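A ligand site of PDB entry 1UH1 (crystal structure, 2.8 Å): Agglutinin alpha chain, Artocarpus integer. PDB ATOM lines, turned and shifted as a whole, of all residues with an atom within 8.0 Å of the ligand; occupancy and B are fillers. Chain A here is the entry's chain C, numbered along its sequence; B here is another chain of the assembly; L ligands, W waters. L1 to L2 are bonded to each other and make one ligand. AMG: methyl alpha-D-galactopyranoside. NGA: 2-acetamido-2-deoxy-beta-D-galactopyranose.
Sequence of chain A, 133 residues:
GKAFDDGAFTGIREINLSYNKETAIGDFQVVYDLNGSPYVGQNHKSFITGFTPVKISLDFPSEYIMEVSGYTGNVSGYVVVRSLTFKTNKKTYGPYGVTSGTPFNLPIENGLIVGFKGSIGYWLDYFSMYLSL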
ATOM      1  N   GLY A   1     -28.033 -21.996   4.525  1.00  0.00           N
ATOM      2  CA  GLY A   1     -26.961 -21.725   3.500  1.00  0.00           C
ATOM      3  C   GLY A   1     -27.362 -22.353   2.167  1.00  0.00           C
ATOM      4  O   GLY A   1     -28.415 -22.912   2.064  1.00  0.00           O
ATOM      5  N   LYS A   2     -26.540 -22.224   1.138  1.00  0.00           N
ATOM      6  CA  LYS A   2     -26.890 -22.808  -0.127  1.00  0.00           C
ATOM      7  C   LYS A   2     -26.333 -24.214  -0.216  1.00  0.00           C
ATOM      8  O   LYS A   2     -25.130 -24.399  -0.062  1.00  0.00           O
ATOM      9  CB  LYS A   2     -26.316 -21.961  -1.231  1.00  0.00           C
ATOM     10  CG  LYS A   2     -26.231 -22.707  -2.493  1.00  0.00           C
ATOM     11  CD  LYS A   2     -26.188 -21.782  -3.601  1.00  0.00           C
ATOM     12  CE  LYS A   2     -26.782 -22.398  -4.816  1.00  0.00           C
ATOM     13  NZ  LYS A   2     -26.252 -21.865  -6.144  1.00  0.00           N
ATOM     14  N   ALA A   3     -27.204 -25.166  -0.525  1.00  0.00           N
ATOM     15  CA  ALA A   3     -26.832 -26.545  -0.635  1.00  0.00           C
ATOM     16  C   ALA A   3     -26.095 -26.884  -1.914  1.00  0.00           C
ATOM     17  O   ALA A   3     -26.252 -26.237  -2.951  1.00  0.00           O
ATOM     18  CB  ALA A   3     -28.059 -27.393  -0.525  1.00  0.00           C
ATOM     19  N   ALA A  24     -15.430 -20.972  11.933  1.00  0.00           N
ATOM     20  CA  ALA A  24     -15.551 -22.338  11.429  1.00  0.00           C
ATOM     21  C   ALA A  24     -15.015 -22.491  10.009  1.00  0.00           C
ATOM     22  O   ALA A  24     -14.209 -21.673   9.545  1.00  0.00           O
ATOM     23  CB  ALA A  24     -16.997 -22.788  11.481  1.00  0.00           C
ATOM     24  N   ILE A  25     -15.462 -23.539   9.319  1.00  0.00           N
ATOM     25  CA  ILE A  25     -15.022 -23.796   7.944  1.00  0.00           C
ATOM     26  C   ILE A  25     -15.773 -22.886   6.965  1.00  0.00           C
ATOM     27  O   ILE A  25     -16.972 -22.685   7.093  1.00  0.00           O
ATOM     28  CB  ILE A  25     -15.263 -25.253   7.545  1.00  0.00           C
ATOM     29  CG1 ILE A  25     -14.470 -26.188   8.470  1.00  0.00           C
ATOM     30  CG2 ILE A  25     -14.860 -25.470   6.084  1.00  0.00           C
ATOM     31  CD1 ILE A  25     -12.974 -26.020   8.371  1.00  0.00           C
ATOM     32  N   SER A  46     -18.462 -19.408   0.754  1.00  0.00           N
ATOM     33  CA  SER A  46     -19.167 -18.813   1.874  1.00  0.00           C
ATOM     34  C   SER A  46     -19.796 -17.502   1.445  1.00  0.00           C
ATOM     35  O   SER A  46     -19.327 -16.851   0.518  1.00  0.00           O
ATOM     36  CB  SER A  46     -18.180 -18.550   3.012  1.00  0.00           C
ATOM     37  OG  SER A  46     -18.703 -17.585   3.913  1.00  0.00           O
ATOM     38  N   PHE A  47     -20.863 -17.108   2.132  1.00  0.00           N
ATOM     39  CA  PHE A  47     -21.544 -15.860   1.826  1.00  0.00           C
ATOM     40  C   PHE A  47     -20.651 -14.681   2.186  1.00  0.00           C
ATOM     41  O   PHE A  47     -20.843 -13.575   1.681  1.00  0.00           O
ATOM     42  CB  PHE A  47     -22.851 -15.751   2.595  1.00  0.00           C
ATOM     43  CG  PHE A  47     -23.906 -16.752   2.170  1.00  0.00           C
ATOM     44  CD1 PHE A  47     -23.760 -17.500   1.007  1.00  0.00           C
ATOM     45  CD2 PHE A  47     -25.073 -16.901   2.913  1.00  0.00           C
ATOM     46  CE1 PHE A  47     -24.763 -18.373   0.591  1.00  0.00           C
ATOM     47  CE2 PHE A  47     -26.071 -17.768   2.510  1.00  0.00           C
ATOM     48  CZ  PHE A  47     -25.919 -18.501   1.352  1.00  0.00           C
ATOM     49  N   ILE A  48     -19.679 -14.933   3.057  1.00  0.00           N
ATOM     50  CA  ILE A  48     -18.739 -13.899   3.498  1.00  0.00           C
ATOM     51  C   ILE A  48     -17.293 -14.258   3.135  1.00  0.00           C
ATOM     52  O   ILE A  48     -17.030 -15.314   2.574  1.00  0.00           O
ATOM     53  CB  ILE A  48     -18.828 -13.687   5.014  1.00  0.00           C
ATOM     54  CG1 ILE A  48     -18.416 -14.964   5.748  1.00  0.00           C
ATOM     55  CG2 ILE A  48     -20.254 -13.284   5.396  1.00  0.00           C
ATOM     56  CD1 ILE A  48     -18.551 -14.878   7.241  1.00  0.00           C
ATOM     57  N   VAL A  75     -22.113 -21.292  16.271  1.00  0.00           N
ATOM     58  CA  VAL A  75     -21.493 -20.028  15.889  1.00  0.00           C
ATOM     59  C   VAL A  75     -22.607 -19.061  15.496  1.00  0.00           C
ATOM     60  O   VAL A  75     -23.323 -19.288  14.527  1.00  0.00           O
ATOM     61  CB  VAL A  75     -20.518 -20.206  14.694  1.00  0.00           C
ATOM     62  CG1 VAL A  75     -19.962 -18.854  14.269  1.00  0.00           C
ATOM     63  CG2 VAL A  75     -19.393 -21.142  15.081  1.00  0.00           C
ATOM     64  N   SER A  76     -22.758 -17.982  16.268  1.00  0.00           N
ATOM     65  CA  SER A  76     -23.807 -16.994  16.044  1.00  0.00           C
ATOM     66  C   SER A  76     -25.152 -17.667  16.031  1.00  0.00           C
ATOM     67  O   SER A  76     -26.040 -17.286  15.277  1.00  0.00           O
ATOM     68  CB  SER A  76     -23.607 -16.248  14.720  1.00  0.00           C
ATOM     69  OG  SER A  76     -22.592 -15.274  14.851  1.00  0.00           O
ATOM     70  N   GLY A  77     -25.290 -18.699  16.851  1.00  0.00           N
ATOM     71  CA  GLY A  77     -26.560 -19.392  16.932  1.00  0.00           C
ATOM     72  C   GLY A  77     -26.832 -20.437  15.865  1.00  0.00           C
ATOM     73  O   GLY A  77     -27.893 -21.046  15.887  1.00  0.00           O
ATOM     74  N   TYR A  78     -25.900 -20.633  14.936  1.00  0.00           N
ATOM     75  CA  TYR A  78     -26.083 -21.631  13.886  1.00  0.00           C
ATOM     76  C   TYR A  78     -25.171 -22.808  14.158  1.00  0.00           C
ATOM     77  O   TYR A  78     -24.017 -22.641  14.532  1.00  0.00           O
ATOM     78  CB  TYR A  78     -25.724 -21.066  12.511  1.00  0.00           C
ATOM     79  CG  TYR A  78     -26.586 -19.909  12.068  1.00  0.00           C
ATOM     80  CD1 TYR A  78     -27.827 -20.117  11.485  1.00  0.00           C
ATOM     81  CD2 TYR A  78     -26.133 -18.599  12.230  1.00  0.00           C
ATOM     82  CE1 TYR A  78     -28.622 -19.040  11.080  1.00  0.00           C
ATOM     83  CE2 TYR A  78     -26.921 -17.508  11.831  1.00  0.00           C
ATOM     84  CZ  TYR A  78     -28.163 -17.738  11.252  1.00  0.00           C
ATOM     85  OH  TYR A  78     -28.943 -16.668  10.862  1.00  0.00           O
ATOM     86  N   VAL A  79     -25.679 -24.015  13.976  1.00  0.00           N
ATOM     87  CA  VAL A  79     -24.850 -25.196  14.170  1.00  0.00           C
ATOM     88  C   VAL A  79     -24.093 -25.414  12.858  1.00  0.00           C
ATOM     89  O   VAL A  79     -24.692 -25.545  11.806  1.00  0.00           O
ATOM     90  CB  VAL A  79     -25.690 -26.439  14.469  1.00  0.00           C
ATOM     91  CG1 VAL A  79     -24.800 -27.649  14.537  1.00  0.00           C
ATOM     92  CG2 VAL A  79     -26.392 -26.255  15.772  1.00  0.00           C
ATOM     93  N   VAL A  80     -22.769 -25.439  12.934  1.00  0.00           N
ATOM     94  CA  VAL A  80     -21.962 -25.610  11.730  1.00  0.00           C
ATOM     95  C   VAL A  80     -20.777 -26.518  11.985  1.00  0.00           C
ATOM     96  O   VAL A  80     -20.521 -26.930  13.116  1.00  0.00           O
ATOM     97  CB  VAL A  80     -21.423 -24.253  11.232  1.00  0.00           C
ATOM     98  CG1 VAL A  80     -22.568 -23.351  10.803  1.00  0.00           C
ATOM     99  CG2 VAL A  80     -20.584 -23.591  12.327  1.00  0.00           C
ATOM    100  N   VAL A  81     -20.056 -26.822  10.915  1.00  0.00           N
ATOM    101  CA  VAL A  81     -18.862 -27.649  11.017  1.00  0.00           C
ATOM    102  C   VAL A  81     -17.737 -26.677  11.321  1.00  0.00           C
ATOM    103  O   VAL A  81     -17.299 -25.926  10.435  1.00  0.00           O
ATOM    104  CB  VAL A  81     -18.600 -28.386   9.683  1.00  0.00           C
ATOM    105  CG1 VAL A  81     -17.355 -29.243   9.800  1.00  0.00           C
ATOM    106  CG2 VAL A  81     -19.799 -29.235   9.328  1.00  0.00           C
ATOM    107  N   SER A 119     -23.908 -28.059   2.637  1.00  0.00           N
ATOM    108  CA  SER A 119     -24.508 -26.737   2.566  1.00  0.00           C
ATOM    109  C   SER A 119     -23.568 -25.693   3.132  1.00  0.00           C
ATOM    110  O   SER A 119     -22.838 -25.951   4.089  1.00  0.00           O
ATOM    111  CB  SER A 119     -25.822 -26.721   3.323  1.00  0.00           C
ATOM    112  OG  SER A 119     -26.368 -25.414   3.344  1.00  0.00           O
ATOM    113  N   ILE A 120     -23.579 -24.503   2.535  1.00  0.00           N
ATOM    114  CA  ILE A 120     -22.708 -23.437   2.994  1.00  0.00           C
ATOM    115  C   ILE A 120     -23.397 -22.090   2.977  1.00  0.00           C
ATOM    116  O   ILE A 120     -23.917 -21.645   1.944  1.00  0.00           O
ATOM    117  CB  ILE A 120     -21.422 -23.346   2.126  1.00  0.00           C
ATOM    118  CG1 ILE A 120     -20.636 -24.651   2.211  1.00  0.00           C
ATOM    119  CG2 ILE A 120     -20.558 -22.181   2.582  1.00  0.00           C
ATOM    120  CD1 ILE A 120     -19.426 -24.682   1.313  1.00  0.00           C
ATOM    121  N   GLY A 121     -23.425 -21.446   4.129  1.00  0.00           N
ATOM    122  CA  GLY A 121     -23.993 -20.117   4.248  1.00  0.00           C
ATOM    123  C   GLY A 121     -22.774 -19.293   4.592  1.00  0.00           C
ATOM    124  O   GLY A 121     -21.892 -19.110   3.758  1.00  0.00           O
ATOM    125  N   TYR A 122     -22.711 -18.794   5.809  1.00  0.00           N
ATOM    126  CA  TYR A 122     -21.540 -18.041   6.229  1.00  0.00           C
ATOM    127  C   TYR A 122     -20.473 -19.098   6.451  1.00  0.00           C
ATOM    128  O   TYR A 122     -19.283 -18.861   6.232  1.00  0.00           O
ATOM    129  CB  TYR A 122     -21.813 -17.313   7.565  1.00  0.00           C
ATOM    130  CG  TYR A 122     -22.478 -15.971   7.422  1.00  0.00           C
ATOM    131  CD1 TYR A 122     -23.437 -15.744   6.449  1.00  0.00           C
ATOM    132  CD2 TYR A 122     -22.148 -14.934   8.283  1.00  0.00           C
ATOM    133  CE1 TYR A 122     -24.074 -14.516   6.334  1.00  0.00           C
ATOM    134  CE2 TYR A 122     -22.772 -13.699   8.185  1.00  0.00           C
ATOM    135  CZ  TYR A 122     -23.724 -13.491   7.203  1.00  0.00           C
ATOM    136  OH  TYR A 122     -24.339 -12.267   7.092  1.00  0.00           O
ATOM    137  N   TRP A 123     -20.915 -20.264   6.889  1.00  0.00           N
ATOM    138  CA  TRP A 123     -20.022 -21.372   7.163  1.00  0.00           C
ATOM    139  C   TRP A 123     -20.608 -22.664   6.640  1.00  0.00           C
ATOM    140  O   TRP A 123     -21.749 -22.706   6.180  1.00  0.00           O
ATOM    141  CB  TRP A 123     -19.794 -21.481   8.673  1.00  0.00           C
ATOM    142  CG  TRP A 123     -19.282 -20.204   9.250  1.00  0.00           C
ATOM    143  CD1 TRP A 123     -18.048 -19.642   9.070  1.00  0.00           C
ATOM    144  CD2 TRP A 123     -20.029 -19.259  10.043  1.00  0.00           C
ATOM    145  NE1 TRP A 123     -17.974 -18.415   9.679  1.00  0.00           N
ATOM    146  CE2 TRP A 123     -19.187 -18.162  10.280  1.00  0.00           C
ATOM    147  CE3 TRP A 123     -21.330 -19.245  10.547  1.00  0.00           C
ATOM    148  CZ2 TRP A 123     -19.596 -17.044  11.033  1.00  0.00           C
ATOM    149  CZ3 TRP A 123     -21.742 -18.135  11.288  1.00  0.00           C
ATOM    150  CH2 TRP A 123     -20.870 -17.053  11.514  1.00  0.00           C
ATOM    151  N   LEU A 124     -19.802 -23.712   6.690  1.00  0.00           N
ATOM    152  CA  LEU A 124     -20.239 -25.018   6.229  1.00  0.00           C
ATOM    153  C   LEU A 124     -21.260 -25.503   7.236  1.00  0.00           C
ATOM    154  O   LEU A 124     -20.926 -25.854   8.363  1.00  0.00           O
ATOM    155  CB  LEU A 124     -19.032 -25.965   6.180  1.00  0.00           C
ATOM    156  CG  LEU A 124     -19.234 -27.435   5.817  1.00  0.00           C
ATOM    157  CD1 LEU A 124     -19.846 -27.584   4.421  1.00  0.00           C
ATOM    158  CD2 LEU A 124     -17.880 -28.114   5.877  1.00  0.00           C
ATOM    159  N   ASP A 125     -22.529 -25.503   6.836  1.00  0.00           N
ATOM    160  CA  ASP A 125     -23.609 -25.933   7.715  1.00  0.00           C
ATOM    161  C   ASP A 125     -23.548 -27.409   8.078  1.00  0.00           C
ATOM    162  O   ASP A 125     -23.703 -27.789   9.245  1.00  0.00           O
ATOM    163  CB  ASP A 125     -24.961 -25.620   7.065  1.00  0.00           C
ATOM    164  CG  ASP A 125     -25.095 -24.167   6.692  1.00  0.00           C
ATOM    165  OD1 ASP A 125     -24.945 -23.310   7.595  1.00  0.00           O
ATOM    166  OD2 ASP A 125     -25.346 -23.856   5.505  1.00  0.00           O
ATOM    167  N   TYR A 126     -23.330 -28.248   7.068  1.00  0.00           N
ATOM    168  CA  TYR A 126     -23.257 -29.684   7.257  1.00  0.00           C
ATOM    169  C   TYR A 126     -22.732 -30.290   5.989  1.00  0.00           C
ATOM    170  O   TYR A 126     -22.633 -29.601   4.959  1.00  0.00           O
ATOM    171  CB  TYR A 126     -24.647 -30.243   7.557  1.00  0.00           C
ATOM    172  CG  TYR A 126     -25.651 -30.002   6.456  1.00  0.00           C
ATOM    173  CD1 TYR A 126     -25.612 -30.732   5.254  1.00  0.00           C
ATOM    174  CD2 TYR A 126     -26.634 -29.026   6.591  1.00  0.00           C
ATOM    175  CE1 TYR A 126     -26.522 -30.479   4.230  1.00  0.00           C
ATOM    176  CE2 TYR A 126     -27.540 -28.765   5.579  1.00  0.00           C
ATOM    177  CZ  TYR A 126     -27.485 -29.490   4.410  1.00  0.00           C
ATOM    178  OH  TYR A 126     -28.384 -29.215   3.405  1.00  0.00           O
ATOM    179  N   ALA B  17     -25.394 -28.925  11.127  1.00  0.00           N
ATOM    180  CA  ALA B  17     -26.773 -28.460  11.310  1.00  0.00           C
ATOM    181  C   ALA B  17     -27.798 -29.561  10.990  1.00  0.00           C
ATOM    182  O   ALA B  17     -27.669 -30.263   9.995  1.00  0.00           O
ATOM    183  CB  ALA B  17     -27.033 -27.249  10.436  1.00  0.00           C
ATOM    184  N   LYS B  18     -28.807 -29.684  11.838  1.00  0.00           N
ATOM    185  CA  LYS B  18     -29.844 -30.691  11.650  1.00  0.00           C
ATOM    186  C   LYS B  18     -30.684 -30.371  10.407  1.00  0.00           C
ATOM    187  O   LYS B  18     -30.722 -31.211   9.486  1.00  0.00           O
ATOM    188  CB  LYS B  18     -30.742 -30.744  12.887  1.00  0.00           C
ATOM    189  CG  LYS B  18     -31.644 -31.969  12.985  1.00  0.00           C
ATOM    190  CD  LYS B  18     -30.892 -33.215  13.452  1.00  0.00           C
ATOM    191  CE  LYS B  18     -29.884 -33.720  12.413  1.00  0.00           C
ATOM    192  NZ  LYS B  18     -30.543 -34.109  11.137  1.00  0.00           N
HETATM  193  C1  AMG L   1     -26.323 -17.755   7.227  1.00  0.00           C
HETATM  194  C2  AMG L   1     -27.406 -18.443   6.557  1.00  0.00           C
HETATM  195  C3  AMG L   1     -27.972 -19.584   7.525  1.00  0.00           C
HETATM  196  C4  AMG L   1     -26.793 -20.539   7.963  1.00  0.00           C
HETATM  197  C5  AMG L   1     -25.645 -19.722   8.561  1.00  0.00           C
HETATM  198  C6  AMG L   1     -24.397 -20.429   9.063  1.00  0.00           C
HETATM  199  C7  AMG L   1     -25.685 -16.026   8.999  1.00  0.00           C
HETATM  200  O1  AMG L   1     -26.651 -16.970   8.405  1.00  0.00           O
HETATM  201  O2  AMG L   1     -28.477 -17.630   6.193  1.00  0.00           O
HETATM  202  O3  AMG L   1     -28.981 -20.297   6.704  1.00  0.00           O
HETATM  203  O4  AMG L   1     -26.424 -21.173   6.752  1.00  0.00           O
HETATM  204  O5  AMG L   1     -25.293 -18.687   7.580  1.00  0.00           O
HETATM  205  O6  AMG L   1     -23.668 -20.907   7.943  1.00  0.00           O
HETATM  206  C1  NGA L   2     -30.080 -20.472   7.162  1.00  0.00           C
HETATM  207  C2  NGA L   2     -31.195 -20.792   6.140  1.00  0.00           C
HETATM  208  C3  NGA L   2     -32.469 -21.190   6.928  1.00  0.00           C
HETATM  209  C4  NGA L   2     -32.188 -22.506   7.803  1.00  0.00           C
HETATM  210  C5  NGA L   2     -31.096 -22.105   8.916  1.00  0.00           C
HETATM  211  C6  NGA L   2     -30.732 -23.272   9.845  1.00  0.00           C
HETATM  212  C7  NGA L   2     -30.570 -19.235   4.235  1.00  0.00           C
HETATM  213  C8  NGA L   2     -30.910 -17.932   3.554  1.00  0.00           C
HETATM  214  N2  NGA L   2     -31.351 -19.604   5.351  1.00  0.00           N
HETATM  215  O3  NGA L   2     -33.446 -21.484   5.985  1.00  0.00           O
HETATM  216  O4  NGA L   2     -31.726 -23.572   6.966  1.00  0.00           O
HETATM  217  O5  NGA L   2     -29.856 -21.623   8.092  1.00  0.00           O
HETATM  218  O6  NGA L   2     -29.604 -22.991  10.704  1.00  0.00           O
HETATM  219  O7  NGA L   2     -29.609 -19.898   3.802  1.00  0.00           O
HETATM  220  O   HOH W   1     -28.417 -24.640  13.034  1.00  0.00           O
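The backbone NH (N) of Gly 1 is in hydrogen-bond range of an oxygen (O7) of NGA L2, at 2.7 Å.
The side-chain carboxylate (OD1) of Asp 125 sits at hydrogen-bond distance from an oxygen (O4) of AMG L1.
An oxygen (O6) of AMG L1 sits at hydrogen-bond distance from the backbone NH of Trp 123 (3.0 Å).
An oxygen (O6) of AMG L1 lies within hydrogen-bond range of the backbone carbonyl oxygen of Trp 123 (3.2 Å).
An oxygen (O5) of AMG L1 is in hydrogen-bond range of the backbone NH (N) of Tyr 122, 3.1 Å away.
OH of Tyr 78 sits close to O1 of AMG L1 (3.4 Å).
CG1 of Val 80 touches C6 of AMG L1, at 3.9 Å.
Gly 121 touches the ligand.
Of the 25 residues printed, 7 come within 4 Å of the ligand.
The backbone NH (N) of Gly 1 lies close to the side-chain carboxylate (OD2) of Asp 125 (3.4 Å).
O of Gly 1 lies close to OG of Ser 119 (3.5 Å).
N of Gly 121 lies within hydrogen-bond range of OD2 of Asp 125, at 3.4 Å.
The backbone carbonyl oxygen of Asp 125 lies within hydrogen-bond range of the backbone NH of Ala 17 of chain B (2.8 Å).
N of Asp 125 is in hydrogen-bond range of O of Ser 119.
O of Tyr 122 sits at hydrogen-bond distance from OG of Ser 46, at 2.7 Å.
The backbone carbonyl oxygen (O) of Gly 121 is in hydrogen-bond range of the backbone NH (N) of Phe 47.
Water W1 lies within hydrogen-bond range of the backbone NH (N) of Val 79 (3.0 Å) and an oxygen (O6) of NGA L2 (3.1 Å).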
